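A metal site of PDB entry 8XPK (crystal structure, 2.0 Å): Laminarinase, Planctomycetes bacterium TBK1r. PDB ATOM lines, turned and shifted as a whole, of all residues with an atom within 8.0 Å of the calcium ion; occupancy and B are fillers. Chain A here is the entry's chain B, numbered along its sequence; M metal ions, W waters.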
ATOM      1  N   PRO A 117     -11.048  30.113 -17.834  1.00  0.00           N
ATOM      2  CA  PRO A 117     -11.533  30.434 -16.488  1.00  0.00           C
ATOM      3  C   PRO A 117     -10.486  30.711 -15.414  1.00  0.00           C
ATOM      4  O   PRO A 117     -10.796  30.672 -14.215  1.00  0.00           O
ATOM      5  CB  PRO A 117     -12.247  29.117 -16.207  1.00  0.00           C
ATOM      6  CG  PRO A 117     -11.252  28.091 -16.658  1.00  0.00           C
ATOM      7  CD  PRO A 117     -10.703  28.683 -17.958  1.00  0.00           C
ATOM      8  N   LYS A 118      -9.236  30.936 -15.827  1.00  0.00           N
ATOM      9  CA  LYS A 118      -8.158  31.185 -14.903  1.00  0.00           C
ATOM     10  C   LYS A 118      -8.425  32.454 -14.106  1.00  0.00           C
ATOM     11  O   LYS A 118      -7.949  32.572 -12.980  1.00  0.00           O
ATOM     12  CB  LYS A 118      -6.818  31.298 -15.654  1.00  0.00           C
ATOM     13  CG  LYS A 118      -6.320  29.991 -16.252  1.00  0.00           C
ATOM     14  CD  LYS A 118      -4.853  29.967 -16.661  1.00  0.00           C
ATOM     15  CE  LYS A 118      -4.463  28.728 -17.403  1.00  0.00           C
ATOM     16  NZ  LYS A 118      -4.724  27.524 -16.608  1.00  0.00           N
ATOM     17  N   CYS A 119      -9.205  33.378 -14.666  1.00  0.00           N
ATOM     18  CA  CYS A 119      -9.587  34.593 -13.976  1.00  0.00           C
ATOM     19  C   CYS A 119     -10.571  34.320 -12.833  1.00  0.00           C
ATOM     20  O   CYS A 119     -10.701  35.134 -11.923  1.00  0.00           O
ATOM     21  CB  CYS A 119     -10.227  35.573 -14.948  1.00  0.00           C
ATOM     22  SG  CYS A 119     -11.721  34.923 -15.730  1.00  0.00           S
ATOM     23  N   GLY A 120     -11.285  33.181 -12.891  1.00  0.00           N
ATOM     24  CA  GLY A 120     -12.298  32.876 -11.907  1.00  0.00           C
ATOM     25  C   GLY A 120     -13.642  33.489 -12.312  1.00  0.00           C
ATOM     26  O   GLY A 120     -13.665  34.581 -12.878  1.00  0.00           O
ATOM     27  N   PHE A 148     -13.598  27.878 -12.768  1.00  0.00           N
ATOM     28  CA  PHE A 148     -12.230  28.273 -12.449  1.00  0.00           C
ATOM     29  C   PHE A 148     -11.270  27.250 -13.022  1.00  0.00           C
ATOM     30  O   PHE A 148     -11.687  26.237 -13.579  1.00  0.00           O
ATOM     31  CB  PHE A 148     -12.035  28.382 -10.939  1.00  0.00           C
ATOM     32  CG  PHE A 148     -12.336  27.130 -10.119  1.00  0.00           C
ATOM     33  CD1 PHE A 148     -13.650  26.795  -9.774  1.00  0.00           C
ATOM     34  CD2 PHE A 148     -11.315  26.300  -9.682  1.00  0.00           C
ATOM     35  CE1 PHE A 148     -13.919  25.665  -9.038  1.00  0.00           C
ATOM     36  CE2 PHE A 148     -11.585  25.165  -8.938  1.00  0.00           C
ATOM     37  CZ  PHE A 148     -12.886  24.853  -8.624  1.00  0.00           C
ATOM     38  N   ALA A 149      -9.964  27.536 -12.880  1.00  0.00           N
ATOM     39  CA  ALA A 149      -8.905  26.609 -13.247  1.00  0.00           C
ATOM     40  C   ALA A 149      -8.569  25.761 -12.016  1.00  0.00           C
ATOM     41  O   ALA A 149      -7.955  26.247 -11.063  1.00  0.00           O
ATOM     42  CB  ALA A 149      -7.699  27.360 -13.766  1.00  0.00           C
ATOM     43  N   GLY A 150      -8.959  24.483 -12.082  1.00  0.00           N
ATOM     44  CA  GLY A 150      -8.840  23.579 -10.943  1.00  0.00           C
ATOM     45  C   GLY A 150      -7.470  22.896 -10.862  1.00  0.00           C
ATOM     46  O   GLY A 150      -6.453  23.448 -11.290  1.00  0.00           O
ATOM     47  N   VAL A 151      -7.445  21.676 -10.323  1.00  0.00           N
ATOM     48  CA  VAL A 151      -6.182  20.978 -10.189  1.00  0.00           C
ATOM     49  C   VAL A 151      -5.647  20.802 -11.614  1.00  0.00           C
ATOM     50  O   VAL A 151      -6.436  20.615 -12.545  1.00  0.00           O
ATOM     51  CB  VAL A 151      -6.222  19.644  -9.404  1.00  0.00           C
ATOM     52  CG1 VAL A 151      -4.824  19.033  -9.261  1.00  0.00           C
ATOM     53  CG2 VAL A 151      -6.833  19.823  -8.020  1.00  0.00           C
ATOM     54  N   GLY A 152      -4.338  21.008 -11.768  1.00  0.00           N
ATOM     55  CA  GLY A 152      -3.684  20.934 -13.065  1.00  0.00           C
ATOM     56  C   GLY A 152      -4.044  22.119 -13.972  1.00  0.00           C
ATOM     57  O   GLY A 152      -3.686  22.144 -15.140  1.00  0.00           O
ATOM     58  N   GLU A 153      -4.766  23.097 -13.422  1.00  0.00           N
ATOM     59  CA  GLU A 153      -5.012  24.372 -14.076  1.00  0.00           C
ATOM     60  C   GLU A 153      -6.055  24.240 -15.184  1.00  0.00           C
ATOM     61  O   GLU A 153      -6.133  25.102 -16.070  1.00  0.00           O
ATOM     62  CB  GLU A 153      -3.708  24.946 -14.635  1.00  0.00           C
ATOM     63  CG  GLU A 153      -2.698  25.337 -13.559  1.00  0.00           C
ATOM     64  CD  GLU A 153      -2.898  26.754 -13.056  1.00  0.00           C
ATOM     65  OE1 GLU A 153      -4.043  27.254 -12.976  1.00  0.00           O
ATOM     66  OE2 GLU A 153      -1.851  27.375 -12.802  1.00  0.00           O
ATOM     67  N   GLN A 154      -6.912  23.206 -15.122  1.00  0.00           N
ATOM     68  CA  GLN A 154      -7.862  22.964 -16.189  1.00  0.00           C
ATOM     69  C   GLN A 154      -9.294  23.279 -15.736  1.00  0.00           C
ATOM     70  O   GLN A 154      -9.636  23.174 -14.572  1.00  0.00           O
ATOM     71  CB  GLN A 154      -7.719  21.527 -16.710  1.00  0.00           C
ATOM     72  CG  GLN A 154      -6.298  21.141 -17.115  1.00  0.00           C
ATOM     73  CD  GLN A 154      -5.747  21.855 -18.343  1.00  0.00           C
ATOM     74  OE1 GLN A 154      -6.455  22.535 -19.100  1.00  0.00           O
ATOM     75  NE2 GLN A 154      -4.461  21.649 -18.575  1.00  0.00           N
ATOM     76  N   THR A 156     -12.740  23.788 -14.402  1.00  0.00           N
ATOM     77  CA  THR A 156     -13.498  23.074 -13.384  1.00  0.00           C
ATOM     78  C   THR A 156     -14.777  23.865 -13.116  1.00  0.00           C
ATOM     79  O   THR A 156     -14.720  25.089 -13.028  1.00  0.00           O
ATOM     80  CB  THR A 156     -12.681  22.929 -12.095  1.00  0.00           C
ATOM     81  OG1 THR A 156     -11.519  22.175 -12.408  1.00  0.00           O
ATOM     82  CG2 THR A 156     -13.441  22.240 -10.988  1.00  0.00           C
ATOM     83  N   ALA A 200      -8.830  26.051  -0.913  1.00  0.00           N
ATOM     84  CA  ALA A 200      -7.893  25.097  -1.503  1.00  0.00           C
ATOM     85  C   ALA A 200      -6.953  25.817  -2.453  1.00  0.00           C
ATOM     86  O   ALA A 200      -7.328  26.808  -3.056  1.00  0.00           O
ATOM     87  CB  ALA A 200      -8.646  23.980  -2.217  1.00  0.00           C
ATOM     88  N   SER A 201      -5.720  25.318  -2.586  1.00  0.00           N
ATOM     89  CA  SER A 201      -4.679  25.991  -3.353  1.00  0.00           C
ATOM     90  C   SER A 201      -5.099  26.239  -4.795  1.00  0.00           C
ATOM     91  O   SER A 201      -4.651  27.203  -5.424  1.00  0.00           O
ATOM     92  CB  SER A 201      -3.373  25.218  -3.279  1.00  0.00           C
ATOM     93  OG  SER A 201      -3.522  23.945  -3.894  1.00  0.00           O
ATOM     94  N   GLU A 202      -5.951  25.374  -5.346  1.00  0.00           N
ATOM     95  CA  GLU A 202      -6.350  25.504  -6.733  1.00  0.00           C
ATOM     96  C   GLU A 202      -7.411  26.591  -6.913  1.00  0.00           C
ATOM     97  O   GLU A 202      -7.753  26.908  -8.059  1.00  0.00           O
ATOM     98  CB  GLU A 202      -6.752  24.175  -7.395  1.00  0.00           C
ATOM     99  CG  GLU A 202      -8.010  23.515  -6.842  1.00  0.00           C
ATOM    100  CD  GLU A 202      -7.767  22.546  -5.687  1.00  0.00           C
ATOM    101  OE1 GLU A 202      -6.688  22.568  -5.040  1.00  0.00           O
ATOM    102  OE2 GLU A 202      -8.704  21.754  -5.442  1.00  0.00           O
ATOM    103  N   MET A 203      -7.854  27.231  -5.831  1.00  0.00           N
ATOM    104  CA  MET A 203      -8.918  28.223  -5.942  1.00  0.00           C
ATOM    105  C   MET A 203      -8.417  29.616  -5.533  1.00  0.00           C
ATOM    106  O   MET A 203      -9.215  30.458  -5.107  1.00  0.00           O
ATOM    107  CB  MET A 203     -10.137  27.801  -5.102  1.00  0.00           C
ATOM    108  CG  MET A 203     -10.768  26.475  -5.549  1.00  0.00           C
ATOM    109  SD  MET A 203     -12.059  25.925  -4.390  1.00  0.00           S
ATOM    110  CE  MET A 203     -13.510  26.721  -5.091  1.00  0.00           C
ATOM    111  N   LYS A 204      -7.117  29.891  -5.739  1.00  0.00           N
ATOM    112  CA  LYS A 204      -6.540  31.180  -5.394  1.00  0.00           C
ATOM    113  C   LYS A 204      -7.144  32.298  -6.257  1.00  0.00           C
ATOM    114  O   LYS A 204      -7.126  33.446  -5.811  1.00  0.00           O
ATOM    115  CB  LYS A 204      -5.012  31.235  -5.526  1.00  0.00           C
ATOM    116  CG  LYS A 204      -4.228  30.609  -4.361  1.00  0.00           C
ATOM    117  CD  LYS A 204      -2.795  31.149  -4.242  1.00  0.00           C
ATOM    118  CE  LYS A 204      -1.897  30.802  -5.403  1.00  0.00           C
ATOM    119  NZ  LYS A 204      -1.501  29.394  -5.386  1.00  0.00           N
ATOM    120  N   GLU A 205      -7.698  31.969  -7.448  1.00  0.00           N
ATOM    121  CA  GLU A 205      -8.435  32.908  -8.274  1.00  0.00           C
ATOM    122  C   GLU A 205      -9.514  33.656  -7.497  1.00  0.00           C
ATOM    123  O   GLU A 205      -9.998  34.675  -7.968  1.00  0.00           O
ATOM    124  CB  GLU A 205      -9.384  32.291  -9.306  1.00  0.00           C
ATOM    125  CG  GLU A 205      -8.756  31.450 -10.388  1.00  0.00           C
ATOM    126  CD  GLU A 205      -8.367  30.044  -9.995  1.00  0.00           C
ATOM    127  OE1 GLU A 205      -7.780  29.817  -8.926  1.00  0.00           O
ATOM    128  OE2 GLU A 205      -8.614  29.193 -10.863  1.00  0.00           O
ATOM    129  N   TYR A 206     -10.000  33.088  -6.382  1.00  0.00           N
ATOM    130  CA  TYR A 206     -11.139  33.662  -5.669  1.00  0.00           C
ATOM    131  C   TYR A 206     -10.666  34.547  -4.529  1.00  0.00           C
ATOM    132  O   TYR A 206     -11.483  34.944  -3.715  1.00  0.00           O
ATOM    133  CB  TYR A 206     -12.077  32.565  -5.171  1.00  0.00           C
ATOM    134  CG  TYR A 206     -12.796  31.885  -6.312  1.00  0.00           C
ATOM    135  CD1 TYR A 206     -13.750  32.573  -7.047  1.00  0.00           C
ATOM    136  CD2 TYR A 206     -12.497  30.595  -6.708  1.00  0.00           C
ATOM    137  CE1 TYR A 206     -14.404  31.990  -8.117  1.00  0.00           C
ATOM    138  CE2 TYR A 206     -13.173  29.993  -7.756  1.00  0.00           C
ATOM    139  CZ  TYR A 206     -14.130  30.686  -8.464  1.00  0.00           C
ATOM    140  OH  TYR A 206     -14.810  30.143  -9.509  1.00  0.00           O
HETATM  141 CA    CA M   1      -6.910  27.838  -9.868  1.00  0.00          CA
HETATM  142  O   HOH W   1      -5.192  28.422  -8.033  1.00  0.00           O
HETATM  143  O   HOH W   2      -5.554  28.963 -11.127  1.00  0.00           O
HETATM  144  O   HOH W   3      -5.388  25.816 -10.036  1.00  0.00           O
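Three residues have an atom within 4 Å of the calcium ion: Ala 149, Glu 202 and Glu 205.
The calcium ion is bound by water W2 (2.2 Å), O of Glu 202 (2.2 Å), O of Ala 149 (2.2 Å), OE1 of Glu 205 (2.4 Å), OE2 of Glu 205 (2.4 Å), water W3 (2.5 Å) and water W1 (2.6 Å). The calcium ion has seven donor atoms within binding distance.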
